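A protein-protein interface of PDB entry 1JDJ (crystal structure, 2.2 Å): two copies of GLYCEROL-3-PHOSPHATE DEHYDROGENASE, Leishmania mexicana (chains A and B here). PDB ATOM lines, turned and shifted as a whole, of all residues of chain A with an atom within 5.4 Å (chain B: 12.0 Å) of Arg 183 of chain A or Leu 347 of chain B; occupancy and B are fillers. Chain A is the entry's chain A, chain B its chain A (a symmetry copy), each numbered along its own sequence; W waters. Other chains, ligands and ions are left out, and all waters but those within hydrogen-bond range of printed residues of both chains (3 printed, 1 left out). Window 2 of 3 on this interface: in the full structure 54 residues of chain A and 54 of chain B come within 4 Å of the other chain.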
ATOM      1  N   LYS A   9     -33.692  17.927   2.218  1.00  0.00           N
ATOM      2  CA  LYS A   9     -33.881  16.469   2.463  1.00  0.00           C
ATOM      3  C   LYS A   9     -32.584  15.713   2.188  1.00  0.00           C
ATOM      4  O   LYS A   9     -32.085  15.703   1.061  1.00  0.00           O
ATOM      5  CB  LYS A   9     -35.001  15.925   1.568  1.00  0.00           C
ATOM      6  CG  LYS A   9     -35.321  14.448   1.785  1.00  0.00           C
ATOM      7  CD  LYS A   9     -35.811  14.157   3.203  1.00  0.00           C
ATOM      8  CE  LYS A   9     -37.210  14.712   3.461  1.00  0.00           C
ATOM      9  NZ  LYS A   9     -37.273  16.200   3.405  1.00  0.00           N
ATOM     10  N   ASP A  10     -32.045  15.085   3.228  1.00  0.00           N
ATOM     11  CA  ASP A  10     -30.800  14.329   3.120  1.00  0.00           C
ATOM     12  C   ASP A  10     -31.067  12.903   2.646  1.00  0.00           C
ATOM     13  O   ASP A  10     -30.197  12.037   2.723  1.00  0.00           O
ATOM     14  CB  ASP A  10     -30.091  14.302   4.477  1.00  0.00           C
ATOM     15  CG  ASP A  10     -29.890  15.692   5.056  1.00  0.00           C
ATOM     16  OD1 ASP A  10     -30.893  16.405   5.264  1.00  0.00           O
ATOM     17  OD2 ASP A  10     -28.728  16.074   5.306  1.00  0.00           O
ATOM     18  N   GLU A  11     -32.279  12.673   2.150  1.00  0.00           N
ATOM     19  CA  GLU A  11     -32.690  11.365   1.657  1.00  0.00           C
ATOM     20  C   GLU A  11     -32.261  11.208   0.198  1.00  0.00           C
ATOM     21  O   GLU A  11     -32.568  12.047  -0.646  1.00  0.00           O
ATOM     22  CB  GLU A  11     -34.209  11.232   1.787  1.00  0.00           C
ATOM     23  CG  GLU A  11     -34.763   9.852   1.511  1.00  0.00           C
ATOM     24  CD  GLU A  11     -36.251   9.773   1.799  1.00  0.00           C
ATOM     25  OE1 GLU A  11     -37.019  10.544   1.186  1.00  0.00           O
ATOM     26  OE2 GLU A  11     -36.654   8.941   2.642  1.00  0.00           O
ATOM     27  N   LEU A  12     -31.551  10.126  -0.096  1.00  0.00           N
ATOM     28  CA  LEU A  12     -31.060   9.885  -1.448  1.00  0.00           C
ATOM     29  C   LEU A  12     -32.154   9.617  -2.473  1.00  0.00           C
ATOM     30  O   LEU A  12     -33.277   9.252  -2.129  1.00  0.00           O
ATOM     31  CB  LEU A  12     -30.073   8.716  -1.444  1.00  0.00           C
ATOM     32  CG  LEU A  12     -28.851   8.853  -0.530  1.00  0.00           C
ATOM     33  CD1 LEU A  12     -27.955   7.627  -0.679  1.00  0.00           C
ATOM     34  CD2 LEU A  12     -28.086  10.114  -0.886  1.00  0.00           C
ATOM     35  N   LEU A  13     -31.808   9.805  -3.741  1.00  0.00           N
ATOM     36  CA  LEU A  13     -32.730   9.571  -4.840  1.00  0.00           C
ATOM     37  C   LEU A  13     -32.141   8.489  -5.726  1.00  0.00           C
ATOM     38  O   LEU A  13     -30.959   8.532  -6.070  1.00  0.00           O
ATOM     39  CB  LEU A  13     -32.923  10.844  -5.676  1.00  0.00           C
ATOM     40  CG  LEU A  13     -33.600  12.066  -5.052  1.00  0.00           C
ATOM     41  CD1 LEU A  13     -33.543  13.235  -6.031  1.00  0.00           C
ATOM     42  CD2 LEU A  13     -35.042  11.733  -4.704  1.00  0.00           C
ATOM     43  N   LYS A  37     -26.813   3.710  -7.801  1.00  0.00           N
ATOM     44  CA  LYS A  37     -27.974   4.566  -7.591  1.00  0.00           C
ATOM     45  C   LYS A  37     -28.958   4.514  -8.759  1.00  0.00           C
ATOM     46  O   LYS A  37     -30.053   5.069  -8.684  1.00  0.00           O
ATOM     47  CB  LYS A  37     -27.508   6.007  -7.383  1.00  0.00           C
ATOM     48  CG  LYS A  37     -26.634   6.209  -6.152  1.00  0.00           C
ATOM     49  CD  LYS A  37     -27.413   5.981  -4.864  1.00  0.00           C
ATOM     50  CE  LYS A  37     -28.634   6.886  -4.782  1.00  0.00           C
ATOM     51  NZ  LYS A  37     -28.274   8.325  -4.953  1.00  0.00           N
ATOM     52  N   ALA A 178     -28.401  22.140  -7.479  1.00  0.00           N
ATOM     53  CA  ALA A 178     -27.228  21.405  -7.027  1.00  0.00           C
ATOM     54  C   ALA A 178     -27.614  20.383  -5.962  1.00  0.00           C
ATOM     55  O   ALA A 178     -27.118  19.257  -5.963  1.00  0.00           O
ATOM     56  CB  ALA A 178     -26.195  22.371  -6.464  1.00  0.00           C
ATOM     57  N   ARG A 179     -28.504  20.782  -5.056  1.00  0.00           N
ATOM     58  CA  ARG A 179     -28.934  19.905  -3.976  1.00  0.00           C
ATOM     59  C   ARG A 179     -29.638  18.656  -4.473  1.00  0.00           C
ATOM     60  O   ARG A 179     -29.527  17.593  -3.859  1.00  0.00           O
ATOM     61  CB  ARG A 179     -29.834  20.663  -2.999  1.00  0.00           C
ATOM     62  CG  ARG A 179     -29.080  21.640  -2.108  1.00  0.00           C
ATOM     63  CD  ARG A 179     -30.044  22.565  -1.396  1.00  0.00           C
ATOM     64  NE  ARG A 179     -29.367  23.540  -0.546  1.00  0.00           N
ATOM     65  CZ  ARG A 179     -29.935  24.661  -0.112  1.00  0.00           C
ATOM     66  NH1 ARG A 179     -31.185  24.940  -0.455  1.00  0.00           N
ATOM     67  NH2 ARG A 179     -29.262  25.499   0.666  1.00  0.00           N
ATOM     68  N   ARG A 180     -30.361  18.767  -5.581  1.00  0.00           N
ATOM     69  CA  ARG A 180     -31.046  17.599  -6.111  1.00  0.00           C
ATOM     70  C   ARG A 180     -30.050  16.639  -6.760  1.00  0.00           C
ATOM     71  O   ARG A 180     -30.160  15.421  -6.611  1.00  0.00           O
ATOM     72  CB  ARG A 180     -32.115  17.998  -7.128  1.00  0.00           C
ATOM     73  CG  ARG A 180     -32.981  16.820  -7.545  1.00  0.00           C
ATOM     74  CD  ARG A 180     -34.045  17.193  -8.559  1.00  0.00           C
ATOM     75  NE  ARG A 180     -34.841  16.026  -8.938  1.00  0.00           N
ATOM     76  CZ  ARG A 180     -35.699  15.405  -8.133  1.00  0.00           C
ATOM     77  NH1 ARG A 180     -35.889  15.840  -6.892  1.00  0.00           N
ATOM     78  NH2 ARG A 180     -36.360  14.340  -8.564  1.00  0.00           N
ATOM     79  N   LEU A 181     -29.078  17.181  -7.485  1.00  0.00           N
ATOM     80  CA  LEU A 181     -28.073  16.341  -8.125  1.00  0.00           C
ATOM     81  C   LEU A 181     -27.242  15.676  -7.034  1.00  0.00           C
ATOM     82  O   LEU A 181     -26.704  14.586  -7.218  1.00  0.00           O
ATOM     83  CB  LEU A 181     -27.172  17.177  -9.037  1.00  0.00           C
ATOM     84  CG  LEU A 181     -27.693  17.436 -10.453  1.00  0.00           C
ATOM     85  CD1 LEU A 181     -27.759  16.115 -11.206  1.00  0.00           C
ATOM     86  CD2 LEU A 181     -29.064  18.092 -10.401  1.00  0.00           C
ATOM     87  N   GLN A 182     -27.154  16.359  -5.900  1.00  0.00           N
ATOM     88  CA  GLN A 182     -26.418  15.894  -4.736  1.00  0.00           C
ATOM     89  C   GLN A 182     -27.107  14.664  -4.136  1.00  0.00           C
ATOM     90  O   GLN A 182     -26.459  13.796  -3.548  1.00  0.00           O
ATOM     91  CB  GLN A 182     -26.343  17.044  -3.726  1.00  0.00           C
ATOM     92  CG  GLN A 182     -26.003  16.682  -2.303  1.00  0.00           C
ATOM     93  CD  GLN A 182     -25.984  17.909  -1.407  1.00  0.00           C
ATOM     94  OE1 GLN A 182     -26.853  18.773  -1.507  1.00  0.00           O
ATOM     95  NE2 GLN A 182     -24.998  17.984  -0.521  1.00  0.00           N
ATOM     96  N   ARG A 183     -28.424  14.595  -4.299  1.00  0.00           N
ATOM     97  CA  ARG A 183     -29.208  13.480  -3.789  1.00  0.00           C
ATOM     98  C   ARG A 183     -29.080  12.289  -4.726  1.00  0.00           C
ATOM     99  O   ARG A 183     -29.245  11.141  -4.320  1.00  0.00           O
ATOM    100  CB  ARG A 183     -30.679  13.883  -3.667  1.00  0.00           C
ATOM    101  CG  ARG A 183     -30.960  14.876  -2.547  1.00  0.00           C
ATOM    102  CD  ARG A 183     -32.148  15.762  -2.891  1.00  0.00           C
ATOM    103  NE  ARG A 183     -33.367  15.003  -3.143  1.00  0.00           N
ATOM    104  CZ  ARG A 183     -34.073  14.390  -2.200  1.00  0.00           C
ATOM    105  NH1 ARG A 183     -33.681  14.446  -0.935  1.00  0.00           N
ATOM    106  NH2 ARG A 183     -35.174  13.725  -2.522  1.00  0.00           N
ATOM    107  N   ILE A 184     -28.773  12.573  -5.986  1.00  0.00           N
ATOM    108  CA  ILE A 184     -28.627  11.532  -6.989  1.00  0.00           C
ATOM    109  C   ILE A 184     -27.226  10.921  -7.017  1.00  0.00           C
ATOM    110  O   ILE A 184     -27.076   9.698  -7.072  1.00  0.00           O
ATOM    111  CB  ILE A 184     -28.960  12.083  -8.394  1.00  0.00           C
ATOM    112  CG1 ILE A 184     -30.437  12.484  -8.450  1.00  0.00           C
ATOM    113  CG2 ILE A 184     -28.629  11.046  -9.460  1.00  0.00           C
ATOM    114  CD1 ILE A 184     -30.826  13.242  -9.706  1.00  0.00           C
ATOM    115  N   MET A 185     -26.207  11.772  -6.972  1.00  0.00           N
ATOM    116  CA  MET A 185     -24.819  11.321  -7.030  1.00  0.00           C
ATOM    117  C   MET A 185     -24.237  10.715  -5.750  1.00  0.00           C
ATOM    118  O   MET A 185     -23.348   9.876  -5.817  1.00  0.00           O
ATOM    119  CB  MET A 185     -23.925  12.469  -7.496  1.00  0.00           C
ATOM    120  CG  MET A 185     -24.260  12.979  -8.881  1.00  0.00           C
ATOM    121  SD  MET A 185     -24.194  11.692 -10.147  1.00  0.00           S
ATOM    122  CE  MET A 185     -22.431  11.411 -10.278  1.00  0.00           C
ATOM    123  N   SER A 186     -24.720  11.146  -4.592  1.00  0.00           N
ATOM    124  CA  SER A 186     -24.225  10.617  -3.324  1.00  0.00           C
ATOM    125  C   SER A 186     -24.657   9.158  -3.145  1.00  0.00           C
ATOM    126  O   SER A 186     -25.839   8.830  -3.289  1.00  0.00           O
ATOM    127  CB  SER A 186     -24.748  11.469  -2.166  1.00  0.00           C
ATOM    128  OG  SER A 186     -24.316  12.809  -2.306  1.00  0.00           O
ATOM    129  N   ARG A 190     -22.238   6.017   1.693  1.00  0.00           N
ATOM    130  CA  ARG A 190     -21.500   7.234   2.026  1.00  0.00           C
ATOM    131  C   ARG A 190     -20.037   7.183   1.591  1.00  0.00           C
ATOM    132  O   ARG A 190     -19.178   7.758   2.247  1.00  0.00           O
ATOM    133  CB  ARG A 190     -21.570   7.506   3.534  1.00  0.00           C
ATOM    134  CG  ARG A 190     -22.988   7.588   4.095  1.00  0.00           C
ATOM    135  CD  ARG A 190     -23.743   8.788   3.550  1.00  0.00           C
ATOM    136  NE  ARG A 190     -23.252  10.047   4.108  1.00  0.00           N
ATOM    137  CZ  ARG A 190     -23.613  11.251   3.676  1.00  0.00           C
ATOM    138  NH1 ARG A 190     -24.472  11.367   2.669  1.00  0.00           N
ATOM    139  NH2 ARG A 190     -23.118  12.341   4.253  1.00  0.00           N
ATOM    140  N   CYS A 194     -21.356  14.260  -1.832  1.00  0.00           N
ATOM    141  CA  CYS A 194     -21.412  15.496  -2.601  1.00  0.00           C
ATOM    142  C   CYS A 194     -21.841  16.693  -1.766  1.00  0.00           C
ATOM    143  O   CYS A 194     -22.730  16.587  -0.929  1.00  0.00           O
ATOM    144  CB  CYS A 194     -22.380  15.330  -3.775  1.00  0.00           C
ATOM    145  SG  CYS A 194     -21.926  14.017  -4.938  1.00  0.00           S
ATOM    146  N   ARG B 236     -11.945  20.227   4.601  1.00  0.00           N
ATOM    147  CA  ARG B 236     -12.948  20.379   5.650  1.00  0.00           C
ATOM    148  C   ARG B 236     -12.277  20.742   6.973  1.00  0.00           C
ATOM    149  O   ARG B 236     -12.849  21.456   7.796  1.00  0.00           O
ATOM    150  CB  ARG B 236     -13.773  19.093   5.817  1.00  0.00           C
ATOM    151  CG  ARG B 236     -14.526  18.628   4.558  1.00  0.00           C
ATOM    152  CD  ARG B 236     -15.475  19.687   4.012  1.00  0.00           C
ATOM    153  NE  ARG B 236     -16.439  20.133   5.015  1.00  0.00           N
ATOM    154  CZ  ARG B 236     -17.311  21.121   4.834  1.00  0.00           C
ATOM    155  NH1 ARG B 236     -17.351  21.776   3.682  1.00  0.00           N
ATOM    156  NH2 ARG B 236     -18.141  21.461   5.811  1.00  0.00           N
ATOM    157  N   ALA B 340     -18.380   7.139  10.601  1.00  0.00           N
ATOM    158  CA  ALA B 340     -19.824   7.091  10.372  1.00  0.00           C
ATOM    159  C   ALA B 340     -20.543   8.221  11.100  1.00  0.00           C
ATOM    160  O   ALA B 340     -21.484   8.809  10.568  1.00  0.00           O
ATOM    161  CB  ALA B 340     -20.387   5.738  10.810  1.00  0.00           C
ATOM    162  N   ASP B 341     -20.108   8.523  12.319  1.00  0.00           N
ATOM    163  CA  ASP B 341     -20.718   9.609  13.076  1.00  0.00           C
ATOM    164  C   ASP B 341     -20.505  10.925  12.332  1.00  0.00           C
ATOM    165  O   ASP B 341     -21.414  11.753  12.241  1.00  0.00           O
ATOM    166  CB  ASP B 341     -20.113   9.690  14.481  1.00  0.00           C
ATOM    167  CG  ASP B 341     -20.534   8.527  15.361  1.00  0.00           C
ATOM    168  OD1 ASP B 341     -20.027   8.412  16.498  1.00  0.00           O
ATOM    169  OD2 ASP B 341     -21.382   7.727  14.914  1.00  0.00           O
ATOM    170  N   LEU B 342     -19.302  11.111  11.797  1.00  0.00           N
ATOM    171  CA  LEU B 342     -18.977  12.319  11.046  1.00  0.00           C
ATOM    172  C   LEU B 342     -19.885  12.486   9.838  1.00  0.00           C
ATOM    173  O   LEU B 342     -20.242  13.605   9.468  1.00  0.00           O
ATOM    174  CB  LEU B 342     -17.529  12.273  10.550  1.00  0.00           C
ATOM    175  CG  LEU B 342     -16.405  12.828  11.418  1.00  0.00           C
ATOM    176  CD1 LEU B 342     -15.087  12.625  10.696  1.00  0.00           C
ATOM    177  CD2 LEU B 342     -16.639  14.310  11.693  1.00  0.00           C
ATOM    178  N   LEU B 343     -20.254  11.367   9.223  1.00  0.00           N
ATOM    179  CA  LEU B 343     -21.093  11.393   8.031  1.00  0.00           C
ATOM    180  C   LEU B 343     -22.592  11.282   8.292  1.00  0.00           C
ATOM    181  O   LEU B 343     -23.388  11.280   7.353  1.00  0.00           O
ATOM    182  CB  LEU B 343     -20.653  10.280   7.082  1.00  0.00           C
ATOM    183  CG  LEU B 343     -19.168  10.308   6.703  1.00  0.00           C
ATOM    184  CD1 LEU B 343     -18.843   9.119   5.821  1.00  0.00           C
ATOM    185  CD2 LEU B 343     -18.838  11.614   5.989  1.00  0.00           C
ATOM    186  N   SER B 344     -22.981  11.199   9.560  1.00  0.00           N
ATOM    187  CA  SER B 344     -24.394  11.081   9.914  1.00  0.00           C
ATOM    188  C   SER B 344     -25.122  12.412   9.769  1.00  0.00           C
ATOM    189  O   SER B 344     -26.347  12.477   9.867  1.00  0.00           O
ATOM    190  CB  SER B 344     -24.533  10.579  11.352  1.00  0.00           C
ATOM    191  OG  SER B 344     -23.948  11.498  12.259  1.00  0.00           O
ATOM    192  N   CYS B 345     -24.357  13.472   9.538  1.00  0.00           N
ATOM    193  CA  CYS B 345     -24.907  14.813   9.384  1.00  0.00           C
ATOM    194  C   CYS B 345     -25.906  14.916   8.233  1.00  0.00           C
ATOM    195  O   CYS B 345     -26.882  15.657   8.315  1.00  0.00           O
ATOM    196  CB  CYS B 345     -23.766  15.812   9.171  1.00  0.00           C
ATOM    197  SG  CYS B 345     -22.598  15.339   7.860  1.00  0.00           S
ATOM    198  N   GLY B 346     -25.658  14.170   7.162  1.00  0.00           N
ATOM    199  CA  GLY B 346     -26.549  14.212   6.018  1.00  0.00           C
ATOM    200  C   GLY B 346     -26.016  15.138   4.939  1.00  0.00           C
ATOM    201  O   GLY B 346     -24.978  15.773   5.120  1.00  0.00           O
ATOM    202  N   LEU B 347     -26.727  15.216   3.818  1.00  0.00           N
ATOM    203  CA  LEU B 347     -26.322  16.063   2.698  1.00  0.00           C
ATOM    204  C   LEU B 347     -26.324  17.534   3.097  1.00  0.00           C
ATOM    205  O   LEU B 347     -27.306  18.033   3.639  1.00  0.00           O
ATOM    206  CB  LEU B 347     -27.271  15.850   1.517  1.00  0.00           C
ATOM    207  CG  LEU B 347     -27.429  14.404   1.042  1.00  0.00           C
ATOM    208  CD1 LEU B 347     -28.423  14.335  -0.108  1.00  0.00           C
ATOM    209  CD2 LEU B 347     -26.084  13.868   0.611  1.00  0.00           C
ATOM    210  N   GLN B 348     -25.226  18.229   2.820  1.00  0.00           N
ATOM    211  CA  GLN B 348     -25.127  19.642   3.169  1.00  0.00           C
ATOM    212  C   GLN B 348     -24.482  20.474   2.070  1.00  0.00           C
ATOM    213  O   GLN B 348     -23.945  19.936   1.093  1.00  0.00           O
ATOM    214  CB  GLN B 348     -24.305  19.810   4.447  1.00  0.00           C
ATOM    215  CG  GLN B 348     -24.783  18.969   5.619  1.00  0.00           C
ATOM    216  CD  GLN B 348     -23.961  19.204   6.870  1.00  0.00           C
ATOM    217  OE1 GLN B 348     -22.743  19.017   6.873  1.00  0.00           O
ATOM    218  NE2 GLN B 348     -24.625  19.616   7.944  1.00  0.00           N
ATOM    219  N   ASP B 349     -24.552  21.793   2.234  1.00  0.00           N
ATOM    220  CA  ASP B 349     -23.929  22.711   1.294  1.00  0.00           C
ATOM    221  C   ASP B 349     -22.484  22.786   1.770  1.00  0.00           C
ATOM    222  O   ASP B 349     -22.203  22.510   2.936  1.00  0.00           O
ATOM    223  CB  ASP B 349     -24.559  24.105   1.364  1.00  0.00           C
ATOM    224  CG  ASP B 349     -26.033  24.104   1.005  1.00  0.00           C
ATOM    225  OD1 ASP B 349     -26.479  23.204   0.259  1.00  0.00           O
ATOM    226  OD2 ASP B 349     -26.743  25.022   1.465  1.00  0.00           O
ATOM    227  N   GLU B 350     -21.575  23.157   0.879  1.00  0.00           N
ATOM    228  CA  GLU B 350     -20.166  23.245   1.240  1.00  0.00           C
ATOM    229  C   GLU B 350     -19.910  24.242   2.367  1.00  0.00           C
ATOM    230  O   GLU B 350     -18.901  24.152   3.067  1.00  0.00           O
ATOM    231  CB  GLU B 350     -19.336  23.598   0.005  1.00  0.00           C
ATOM    232  CG  GLU B 350     -17.835  23.574   0.232  1.00  0.00           C
ATOM    233  CD  GLU B 350     -17.073  23.245  -1.034  1.00  0.00           C
ATOM    234  OE1 GLU B 350     -17.386  23.833  -2.094  1.00  0.00           O
ATOM    235  OE2 GLU B 350     -16.154  22.402  -0.968  1.00  0.00           O
ATOM    236  N   GLY B 351     -20.817  25.194   2.543  1.00  0.00           N
ATOM    237  CA  GLY B 351     -20.657  26.162   3.619  1.00  0.00           C
ATOM    238  C   GLY B 351     -19.572  27.228   3.504  1.00  0.00           C
ATOM    239  O   GLY B 351     -19.043  27.695   4.521  1.00  0.00           O
HETATM  240  O   HOH W   1     -22.788  16.636   1.781  1.00  0.00           O
HETATM  241  O   HOH W   2     -25.262   8.608   6.557  1.00  0.00           O
HETATM  242  O   HOH W   3     -22.191  15.216   4.693  1.00  0.00           O
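The guanidinium group (NH2) of Arg 190 of chain A is in hydrogen-bond range of the backbone carbonyl oxygen (O) of Leu 343 of chain B.
The side-chain amide nitrogen of Gln 182 of chain A is in hydrogen-bond range of the backbone carbonyl oxygen of Gln 348 of chain B, 2.7 Å away.
NH2 of Arg 179 of chain A lies within salt-bridge range of OD2 of Asp 349 of chain B (2.7 Å).
N of Leu 347 of chain B sits at hydrogen-bond distance from OD2 of Asp 10 of chain A (2.6 Å).
The side-chain amino group of Lys 37 of chain A is in hydrogen-bond range of the backbone carbonyl oxygen of Arg 183 of chain A (3.0 Å).
The backbone carbonyl oxygen (O) of Lys 9 of chain A lies within hydrogen-bond range of the guanidinium group (NH1) of Arg 183 of chain A (2.8 Å).
The backbone carbonyl oxygen (O) of Leu 342 of chain B sits at hydrogen-bond distance from the side-chain sulfur (SG) of Cys 345 of chain B (3.3 Å).
The backbone carbonyl oxygen (O) of Glu 11 of chain A is in hydrogen-bond range of the guanidinium group (NH1) of Arg 183 of chain A (2.7 Å).
The backbone carbonyl oxygen (O) of Ser 186 of chain A lies within hydrogen-bond range of the side-chain amino group (NZ) of Lys 37 of chain A (3.0 Å).
N of Leu 13 of chain A sits at hydrogen-bond distance from O of Arg 183 of chain A, 2.9 Å away.
Among the printed residues, pairs that only touch across the chains: Asp 10 of chain A with Cys 345 of chain B (3.6 Å), Asp 10 of chain A with Gly 346 of chain B (2.9 Å), Gln 182 of chain A with Leu 347 of chain B (3.7 Å), Arg 183 of chain A with Leu 347 of chain B (3.6 Å), Ser 186 of chain A with Leu 347 of chain B (3.6 Å), Arg 190 of chain A with Gly 346 of chain B (3.999 Å) and Arg 190 of chain A with Leu 347 of chain B (3.6 Å).
No residue of chain B comes within 4 Å of Lys 9 of chain A.
Asp 10 of chain A touches just these residues of chain B: Cys 345, Gly 346 and Leu 347.
Leu 13 of chain A touches none of the printed residues of chain B.
No residue of chain B comes within 4 Å of Leu 181 of chain A.
Arg 183 of chain A touches one residue of chain B.
Ser 186 of chain A touches just one residue of chain B: Leu 347 (3.6 Å).
Of the printed residues of chain B, Arg 190 of chain A touches Leu 343 (3.3 Å), Gly 346 (3.999 Å) and Leu 347 (3.6 Å).
No residue of chain B comes within 4 Å of Cys 194 of chain A.
Printed residues of chain A within 4 Å of Cys 345 of chain B: Asp 10.
Of the printed residues of chain A, Leu 347 of chain B touches Asp 10 (2.6 Å), Gln 182 (3.7 Å), Arg 183 (3.6 Å), Ser 186 (3.6 Å) and Arg 190 (3.6 Å).
Of the printed residues of chain A, Gln 348 of chain B touches Gln 182.
Gly 351 of chain B touches none of the printed residues of chain A.
The nearest residue of chain B that does not touch Arg 183 of chain A is Gln 348 of chain B (8.5 Å).
The nearest residue of chain A that does not touch Leu 347 of chain B is Lys 9 of chain A (4.1 Å).
Of the 17 printed residues of chain A, 6 touch a printed residue of chain B.
Among the printed residues, Asp or Glu carboxylates within 4 Å of a Lys or Arg side-chain nitrogen of the other chain: Arg 179 of chain A with Asp 349 of chain B (2.7 Å).
No position is printed for both chains.
Of the 11 pairs that touch across the chains among the printed residues, none has its exchanged pair printed and touching as well.
Water W1 lies within hydrogen-bond range of O of Cys 194 of chain A (2.7 Å), N of Gln 348 of chain B (3.1 Å) and NE2 of Gln 182 of chain A (3.5 Å).
Water W3 lies within hydrogen-bond range of O of Gly 346 of chain B (2.9 Å), NH2 of Arg 190 of chain A (3.1 Å) and SG of Cys 345 of chain B (3.2 Å).
Water W2 bridges the backbone carbonyl oxygen (O) of Leu 343 of chain B (3.4 Å) and the guanidinium group (NE) of Arg 190 of chain A (3.5 Å).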
